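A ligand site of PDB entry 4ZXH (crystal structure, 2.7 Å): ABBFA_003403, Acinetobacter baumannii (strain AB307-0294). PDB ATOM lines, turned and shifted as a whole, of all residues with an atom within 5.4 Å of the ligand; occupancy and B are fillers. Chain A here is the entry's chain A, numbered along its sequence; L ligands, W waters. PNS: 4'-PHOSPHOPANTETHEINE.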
ATOM      1  N   LEU A  24      19.830 -25.969  11.869  1.00  0.00           N
ATOM      2  CA  LEU A  24      20.098 -26.911  10.810  1.00  0.00           C
ATOM      3  C   LEU A  24      20.913 -26.303   9.661  1.00  0.00           C
ATOM      4  O   LEU A  24      21.902 -26.882   9.216  1.00  0.00           O
ATOM      5  CB  LEU A  24      18.782 -27.465  10.285  1.00  0.00           C
ATOM      6  CG  LEU A  24      18.741 -28.208   8.959  1.00  0.00           C
ATOM      7  CD1 LEU A  24      19.661 -29.395   9.011  1.00  0.00           C
ATOM      8  CD2 LEU A  24      17.295 -28.637   8.701  1.00  0.00           C
ATOM      9  N   GLY A  25      20.506 -25.127   9.212  1.00  0.00           N
ATOM     10  CA  GLY A  25      21.173 -24.502   8.081  1.00  0.00           C
ATOM     11  C   GLY A  25      22.633 -24.157   8.353  1.00  0.00           C
ATOM     12  O   GLY A  25      23.495 -24.429   7.518  1.00  0.00           O
ATOM     13  N   ILE A  26      22.908 -23.545   9.493  1.00  0.00           N
ATOM     14  CA  ILE A  26      24.292 -23.235   9.832  1.00  0.00           C
ATOM     15  C   ILE A  26      25.110 -24.510   9.982  1.00  0.00           C
ATOM     16  O   ILE A  26      26.213 -24.630   9.446  1.00  0.00           O
ATOM     17  CB  ILE A  26      24.414 -22.468  11.142  1.00  0.00           C
ATOM     18  CG1 ILE A  26      23.440 -21.282  11.208  1.00  0.00           C
ATOM     19  CG2 ILE A  26      25.856 -22.099  11.354  1.00  0.00           C
ATOM     20  CD1 ILE A  26      23.673 -20.256  10.183  1.00  0.00           C
ATOM     21  N   TYR A  28      24.605 -27.498   8.792  1.00  0.00           N
ATOM     22  CA  TYR A  28      24.824 -28.102   7.485  1.00  0.00           C
ATOM     23  C   TYR A  28      25.976 -27.440   6.722  1.00  0.00           C
ATOM     24  O   TYR A  28      26.851 -28.116   6.185  1.00  0.00           O
ATOM     25  CB  TYR A  28      23.537 -28.039   6.655  1.00  0.00           C
ATOM     26  CG  TYR A  28      23.644 -28.712   5.309  1.00  0.00           C
ATOM     27  CD1 TYR A  28      23.621 -30.097   5.198  1.00  0.00           C
ATOM     28  CD2 TYR A  28      23.748 -27.965   4.158  1.00  0.00           C
ATOM     29  CE1 TYR A  28      23.709 -30.719   3.950  1.00  0.00           C
ATOM     30  CE2 TYR A  28      23.844 -28.572   2.924  1.00  0.00           C
ATOM     31  CZ  TYR A  28      23.829 -29.946   2.819  1.00  0.00           C
ATOM     32  OH  TYR A  28      23.921 -30.527   1.559  1.00  0.00           O
ATOM     33  N   ILE A  29      25.970 -26.113   6.671  1.00  0.00           N
ATOM     34  CA  ILE A  29      27.005 -25.397   5.938  1.00  0.00           C
ATOM     35  C   ILE A  29      28.395 -25.733   6.494  1.00  0.00           C
ATOM     36  O   ILE A  29      29.341 -25.937   5.722  1.00  0.00           O
ATOM     37  CB  ILE A  29      26.731 -23.871   5.954  1.00  0.00           C
ATOM     38  CG1 ILE A  29      25.433 -23.590   5.219  1.00  0.00           C
ATOM     39  CG2 ILE A  29      27.862 -23.101   5.292  1.00  0.00           C
ATOM     40  CD1 ILE A  29      25.010 -22.157   5.188  1.00  0.00           C
ATOM     41  N   TYR A  39      30.873 -18.341  10.125  1.00  0.00           N
ATOM     42  CA  TYR A  39      29.899 -18.289  11.213  1.00  0.00           C
ATOM     43  C   TYR A  39      30.544 -18.306  12.621  1.00  0.00           C
ATOM     44  O   TYR A  39      29.892 -18.639  13.609  1.00  0.00           O
ATOM     45  CB  TYR A  39      28.890 -19.426  11.069  1.00  0.00           C
ATOM     46  CG  TYR A  39      28.020 -19.245   9.862  1.00  0.00           C
ATOM     47  CD1 TYR A  39      26.926 -18.383   9.897  1.00  0.00           C
ATOM     48  CD2 TYR A  39      28.302 -19.908   8.667  1.00  0.00           C
ATOM     49  CE1 TYR A  39      26.133 -18.189   8.773  1.00  0.00           C
ATOM     50  CE2 TYR A  39      27.518 -19.708   7.539  1.00  0.00           C
ATOM     51  CZ  TYR A  39      26.437 -18.849   7.598  1.00  0.00           C
ATOM     52  OH  TYR A  39      25.629 -18.661   6.489  1.00  0.00           O
ATOM     53  N   ALA A 279      18.302 -11.281   1.394  1.00  0.00           N
ATOM     54  CA  ALA A 279      18.019 -12.021   2.626  1.00  0.00           C
ATOM     55  C   ALA A 279      18.111 -11.077   3.825  1.00  0.00           C
ATOM     56  O   ALA A 279      19.015 -10.253   3.874  1.00  0.00           O
ATOM     57  CB  ALA A 279      18.974 -13.195   2.807  1.00  0.00           C
ATOM     58  N   PRO A 281      17.875 -11.658   8.024  1.00  0.00           N
ATOM     59  CA  PRO A 281      17.740 -12.229   9.364  1.00  0.00           C
ATOM     60  C   PRO A 281      16.731 -11.513  10.261  1.00  0.00           C
ATOM     61  O   PRO A 281      16.735 -10.284  10.311  1.00  0.00           O
ATOM     62  CB  PRO A 281      19.139 -12.072   9.939  1.00  0.00           C
ATOM     63  CG  PRO A 281      20.008 -12.297   8.744  1.00  0.00           C
ATOM     64  CD  PRO A 281      19.266 -11.722   7.552  1.00  0.00           C
ATOM     65  N   THR A 300      16.599 -16.604   8.690  1.00  0.00           N
ATOM     66  CA  THR A 300      16.741 -15.842   7.472  1.00  0.00           C
ATOM     67  C   THR A 300      15.373 -15.773   6.768  1.00  0.00           C
ATOM     68  O   THR A 300      14.645 -16.765   6.729  1.00  0.00           O
ATOM     69  CB  THR A 300      17.793 -16.481   6.530  1.00  0.00           C
ATOM     70  OG1 THR A 300      19.057 -16.542   7.187  1.00  0.00           O
ATOM     71  CG2 THR A 300      17.955 -15.684   5.235  1.00  0.00           C
ATOM     72  N   PHE A 335      14.106 -20.851   7.175  1.00  0.00           N
ATOM     73  CA  PHE A 335      14.629 -20.698   5.833  1.00  0.00           C
ATOM     74  C   PHE A 335      14.870 -22.057   5.171  1.00  0.00           C
ATOM     75  O   PHE A 335      14.600 -22.229   3.988  1.00  0.00           O
ATOM     76  CB  PHE A 335      15.924 -19.894   5.848  1.00  0.00           C
ATOM     77  CG  PHE A 335      16.461 -19.590   4.488  1.00  0.00           C
ATOM     78  CD1 PHE A 335      15.739 -18.792   3.618  1.00  0.00           C
ATOM     79  CD2 PHE A 335      17.684 -20.076   4.076  1.00  0.00           C
ATOM     80  CE1 PHE A 335      16.208 -18.510   2.364  1.00  0.00           C
ATOM     81  CE2 PHE A 335      18.174 -19.797   2.835  1.00  0.00           C
ATOM     82  CZ  PHE A 335      17.436 -19.010   1.971  1.00  0.00           C
ATOM     83  N   SER A 336      15.353 -23.016   5.943  1.00  0.00           N
ATOM     84  CA  SER A 336      15.629 -24.344   5.413  1.00  0.00           C
ATOM     85  C   SER A 336      14.361 -24.993   4.929  1.00  0.00           C
ATOM     86  O   SER A 336      14.356 -25.715   3.936  1.00  0.00           O
ATOM     87  CB  SER A 336      16.325 -25.233   6.462  1.00  0.00           C
ATOM     88  OG  SER A 336      15.455 -25.515   7.542  1.00  0.00           O
ATOM     89  N   VAL A 339      13.501 -23.430   1.535  1.00  0.00           N
ATOM     90  CA  VAL A 339      14.302 -23.913   0.420  1.00  0.00           C
ATOM     91  C   VAL A 339      13.817 -25.293   0.031  1.00  0.00           C
ATOM     92  O   VAL A 339      13.746 -25.617  -1.152  1.00  0.00           O
ATOM     93  CB  VAL A 339      15.782 -23.943   0.754  1.00  0.00           C
ATOM     94  CG1 VAL A 339      16.521 -24.842  -0.228  1.00  0.00           C
ATOM     95  CG2 VAL A 339      16.351 -22.544   0.704  1.00  0.00           C
ATOM     96  N   GLU A 340      13.449 -26.094   1.024  1.00  0.00           N
ATOM     97  CA  GLU A 340      12.874 -27.410   0.774  1.00  0.00           C
ATOM     98  C   GLU A 340      11.605 -27.317  -0.085  1.00  0.00           C
ATOM     99  O   GLU A 340      11.420 -28.118  -0.994  1.00  0.00           O
ATOM    100  CB  GLU A 340      12.591 -28.130   2.098  1.00  0.00           C
ATOM    101  CG  GLU A 340      11.760 -29.410   2.007  1.00  0.00           C
ATOM    102  CD  GLU A 340      11.570 -30.107   3.373  1.00  0.00           C
ATOM    103  OE1 GLU A 340      12.166 -29.673   4.388  1.00  0.00           O
ATOM    104  OE2 GLU A 340      10.818 -31.100   3.427  1.00  0.00           O
ATOM    105  N   ARG A 346      19.952 -27.090  -6.737  1.00  0.00           N
ATOM    106  CA  ARG A 346      21.061 -26.985  -5.802  1.00  0.00           C
ATOM    107  C   ARG A 346      22.364 -26.761  -6.574  1.00  0.00           C
ATOM    108  O   ARG A 346      22.598 -27.370  -7.614  1.00  0.00           O
ATOM    109  CB  ARG A 346      21.147 -28.217  -4.922  1.00  0.00           C
ATOM    110  CG  ARG A 346      19.888 -28.478  -4.108  1.00  0.00           C
ATOM    111  CD  ARG A 346      19.429 -27.282  -3.256  1.00  0.00           C
ATOM    112  NE  ARG A 346      18.543 -27.743  -2.178  1.00  0.00           N
ATOM    113  CZ  ARG A 346      17.284 -28.132  -2.361  1.00  0.00           C
ATOM    114  NH1 ARG A 346      16.749 -28.097  -3.574  1.00  0.00           N
ATOM    115  NH2 ARG A 346      16.558 -28.561  -1.339  1.00  0.00           N
ATOM    116  N   ASN A 351      24.734 -19.586  -2.254  1.00  0.00           N
ATOM    117  CA  ASN A 351      23.710 -19.874  -1.270  1.00  0.00           C
ATOM    118  C   ASN A 351      22.341 -19.888  -1.962  1.00  0.00           C
ATOM    119  O   ASN A 351      22.044 -19.006  -2.764  1.00  0.00           O
ATOM    120  CB  ASN A 351      23.745 -18.867  -0.128  1.00  0.00           C
ATOM    121  CG  ASN A 351      22.692 -19.140   0.905  1.00  0.00           C
ATOM    122  OD1 ASN A 351      22.854 -20.025   1.748  1.00  0.00           O
ATOM    123  ND2 ASN A 351      21.589 -18.406   0.829  1.00  0.00           N
ATOM    124  N   PRO A 352      21.517 -20.908  -1.695  1.00  0.00           N
ATOM    125  CA  PRO A 352      20.197 -21.077  -2.323  1.00  0.00           C
ATOM    126  C   PRO A 352      19.303 -19.848  -2.180  1.00  0.00           C
ATOM    127  O   PRO A 352      19.339 -19.236  -1.114  1.00  0.00           O
ATOM    128  CB  PRO A 352      19.595 -22.249  -1.550  1.00  0.00           C
ATOM    129  CG  PRO A 352      20.769 -23.039  -1.099  1.00  0.00           C
ATOM    130  CD  PRO A 352      21.875 -22.051  -0.826  1.00  0.00           C
ATOM    131  N   GLY A 357      22.624 -10.018   1.310  1.00  0.00           N
ATOM    132  CA  GLY A 357      21.977  -9.899   2.605  1.00  0.00           C
ATOM    133  C   GLY A 357      22.039  -8.513   3.198  1.00  0.00           C
ATOM    134  O   GLY A 357      22.876  -7.687   2.822  1.00  0.00           O
ATOM    135  N   PHE A 359      21.674  -7.027   7.286  1.00  0.00           N
ATOM    136  CA  PHE A 359      21.400  -7.222   8.715  1.00  0.00           C
ATOM    137  C   PHE A 359      21.268  -5.854   9.311  1.00  0.00           C
ATOM    138  O   PHE A 359      22.072  -4.977   9.034  1.00  0.00           O
ATOM    139  CB  PHE A 359      22.521  -7.963   9.485  1.00  0.00           C
ATOM    140  CG  PHE A 359      23.012  -9.228   8.833  1.00  0.00           C
ATOM    141  CD1 PHE A 359      22.273  -9.888   7.869  1.00  0.00           C
ATOM    142  CD2 PHE A 359      24.223  -9.777   9.227  1.00  0.00           C
ATOM    143  CE1 PHE A 359      22.749 -11.059   7.279  1.00  0.00           C
ATOM    144  CE2 PHE A 359      24.706 -10.955   8.640  1.00  0.00           C
ATOM    145  CZ  PHE A 359      23.962 -11.595   7.666  1.00  0.00           C
ATOM    146  N   GLN A 400      29.694 -15.244   4.329  1.00  0.00           N
ATOM    147  CA  GLN A 400      28.440 -15.970   4.417  1.00  0.00           C
ATOM    148  C   GLN A 400      27.731 -15.925   3.088  1.00  0.00           C
ATOM    149  O   GLN A 400      27.211 -16.939   2.619  1.00  0.00           O
ATOM    150  CB  GLN A 400      27.549 -15.394   5.505  1.00  0.00           C
ATOM    151  CG  GLN A 400      28.039 -15.717   6.894  1.00  0.00           C
ATOM    152  CD  GLN A 400      27.264 -14.966   7.938  1.00  0.00           C
ATOM    153  OE1 GLN A 400      26.331 -14.222   7.610  1.00  0.00           O
ATOM    154  NE2 GLN A 400      27.619 -15.167   9.215  1.00  0.00           N
ATOM    155  N   LEU A 401      27.720 -14.734   2.493  1.00  0.00           N
ATOM    156  CA  LEU A 401      27.028 -14.489   1.234  1.00  0.00           C
ATOM    157  C   LEU A 401      27.956 -13.846   0.224  1.00  0.00           C
ATOM    158  O   LEU A 401      29.147 -13.726   0.469  1.00  0.00           O
ATOM    159  CB  LEU A 401      25.809 -13.611   1.458  1.00  0.00           C
ATOM    160  CG  LEU A 401      24.732 -14.186   2.388  1.00  0.00           C
ATOM    161  CD1 LEU A 401      23.636 -13.141   2.572  1.00  0.00           C
ATOM    162  CD2 LEU A 401      24.179 -15.507   1.818  1.00  0.00           C
ATOM    163  N   PHE A1002      18.566 -34.425  -5.507  1.00  0.00           N
ATOM    164  CA  PHE A1002      17.861 -33.229  -5.074  1.00  0.00           C
ATOM    165  C   PHE A1002      16.708 -32.898  -6.024  1.00  0.00           C
ATOM    166  O   PHE A1002      15.686 -32.373  -5.593  1.00  0.00           O
ATOM    167  CB  PHE A1002      18.845 -32.060  -4.935  1.00  0.00           C
ATOM    168  CG  PHE A1002      19.885 -32.271  -3.865  1.00  0.00           C
ATOM    169  CD1 PHE A1002      19.614 -31.926  -2.536  1.00  0.00           C
ATOM    170  CD2 PHE A1002      21.114 -32.832  -4.178  1.00  0.00           C
ATOM    171  CE1 PHE A1002      20.563 -32.140  -1.531  1.00  0.00           C
ATOM    172  CE2 PHE A1002      22.079 -33.035  -3.180  1.00  0.00           C
ATOM    173  CZ  PHE A1002      21.799 -32.700  -1.856  1.00  0.00           C
ATOM    174  N   HIS A1007      16.636 -33.054  -0.046  1.00  0.00           N
ATOM    175  CA  HIS A1007      17.069 -31.751   0.457  1.00  0.00           C
ATOM    176  C   HIS A1007      18.121 -31.912   1.544  1.00  0.00           C
ATOM    177  O   HIS A1007      18.458 -33.019   1.944  1.00  0.00           O
ATOM    178  CB  HIS A1007      15.884 -30.966   0.998  1.00  0.00           C
ATOM    179  CG  HIS A1007      15.093 -31.722   2.022  1.00  0.00           C
ATOM    180  ND1 HIS A1007      15.503 -31.849   3.337  1.00  0.00           N
ATOM    181  CD2 HIS A1007      13.939 -32.413   1.916  1.00  0.00           C
ATOM    182  CE1 HIS A1007      14.626 -32.572   4.000  1.00  0.00           C
ATOM    183  NE2 HIS A1007      13.662 -32.928   3.170  1.00  0.00           N
ATOM    184  N   SER A1008      18.595 -30.785   2.030  1.00  0.00           N
ATOM    185  CA  SER A1008      19.762 -30.753   2.890  1.00  0.00           C
ATOM    186  C   SER A1008      19.724 -31.684   4.132  1.00  0.00           C
ATOM    187  O   SER A1008      20.659 -32.449   4.311  1.00  0.00           O
ATOM    188  CB  SER A1008      20.025 -29.313   3.285  1.00  0.00           C
ATOM    189  OG  SER A1008      20.603 -28.661   2.141  1.00  0.00           O
ATOM    190  N   LEU A1009      18.675 -31.673   4.947  1.00  0.00           N
ATOM    191  CA  LEU A1009      18.625 -32.625   6.063  1.00  0.00           C
ATOM    192  C   LEU A1009      18.668 -34.082   5.566  1.00  0.00           C
ATOM    193  O   LEU A1009      19.426 -34.896   6.099  1.00  0.00           O
ATOM    194  CB  LEU A1009      17.372 -32.414   6.920  1.00  0.00           C
ATOM    195  CG  LEU A1009      17.201 -33.346   8.120  1.00  0.00           C
ATOM    196  CD1 LEU A1009      18.512 -33.481   8.886  1.00  0.00           C
ATOM    197  CD2 LEU A1009      16.083 -32.888   9.063  1.00  0.00           C
HETATM  198  O23 PNS L   1      20.365 -27.149   0.105  1.00  0.00           O
HETATM  199  P24 PNS L   1      19.652 -27.629   1.339  1.00  0.00           P
HETATM  200  O25 PNS L   1      18.280 -28.226   1.185  1.00  0.00           O
HETATM  201  O27 PNS L   1      19.519 -26.326   2.282  1.00  0.00           O
HETATM  202  C28 PNS L   1      20.679 -25.579   2.644  1.00  0.00           C
HETATM  203  C29 PNS L   1      20.267 -24.459   3.573  1.00  0.00           C
HETATM  204  C30 PNS L   1      19.586 -25.141   4.760  1.00  0.00           C
HETATM  205  C31 PNS L   1      19.291 -23.526   2.851  1.00  0.00           C
HETATM  206  C32 PNS L   1      21.502 -23.655   3.992  1.00  0.00           C
HETATM  207  O33 PNS L   1      22.271 -23.411   2.798  1.00  0.00           O
HETATM  208  C34 PNS L   1      21.104 -22.367   4.687  1.00  0.00           C
HETATM  209  O35 PNS L   1      20.475 -22.360   5.746  1.00  0.00           O
HETATM  210  N36 PNS L   1      21.464 -21.214   4.138  1.00  0.00           N
HETATM  211  C37 PNS L   1      21.133 -19.934   4.732  1.00  0.00           C
HETATM  212  C38 PNS L   1      22.442 -19.200   5.028  1.00  0.00           C
HETATM  213  C39 PNS L   1      22.283 -18.347   6.251  1.00  0.00           C
HETATM  214  O40 PNS L   1      21.600 -18.724   7.184  1.00  0.00           O
HETATM  215  N41 PNS L   1      22.915 -17.191   6.187  1.00  0.00           N
HETATM  216  C42 PNS L   1      22.978 -16.149   7.182  1.00  0.00           C
HETATM  217  C43 PNS L   1      23.557 -14.996   6.386  1.00  0.00           C
HETATM  218  S44 PNS L   1      22.187 -13.960   5.857  1.00  0.00           S
HETATM  219  O   HOH W   1      19.159 -20.937   7.883  1.00  0.00           O
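An oxygen (O25) of the ligand is in hydrogen-bond range of the backbone NH (N) of Ser 1008 (2.7 Å). The side-chain hydroxyl (OG) of Ser 1008 is bonded to a phosphorus (P24) of the ligand (1.6 Å). An oxygen (O23) of the ligand lies within hydrogen-bond range of the guanidinium group (NE) of Arg 346 (3.0 Å). A nitrogen (N36) of the ligand lies within hydrogen-bond range of the side-chain amide oxygen of Asn 351 (3.0 Å). The side-chain hydroxyl (OH) of Tyr 39 sits at hydrogen-bond distance from a nitrogen (N41) of the ligand. OG1 of Thr 300 sits at hydrogen-bond distance from O40 of the ligand, at 3.4 Å.
The side-chain carboxylate (OE2) of Glu 340 is in hydrogen-bond range of a ring nitrogen (NE2) of His 1007, at 3.4 Å.
CA of Gly 25 touches O35 of the ligand (3.2 Å). CD1 of Ile 26 touches O40 of the ligand, at 3.95 Å. Ile 29 touches the ligand (CD1 to N36, 3.8 Å). Pro 281 touches the ligand. Phe 335 touches the ligand. Ser 336 touches the ligand. Val 339 touches the ligand (CG2 to C31, 3.8 Å). Pro 352 touches the ligand. Phe 359 touches the ligand (CE1 to S44, 3.3 Å). OE1 of Gln 400 touches C43 of the ligand, at 3.1 Å. Leu 401 touches the ligand. CB of His 1007 touches O25 of the ligand, at 3.6 Å. Hydrophobic or aromatic side chains within 4 Å of the ligand: Ile 26, Ile 29, Pro 281, Phe 335, Val 339, Pro 352, Phe 359, Leu 401 and His 1007.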
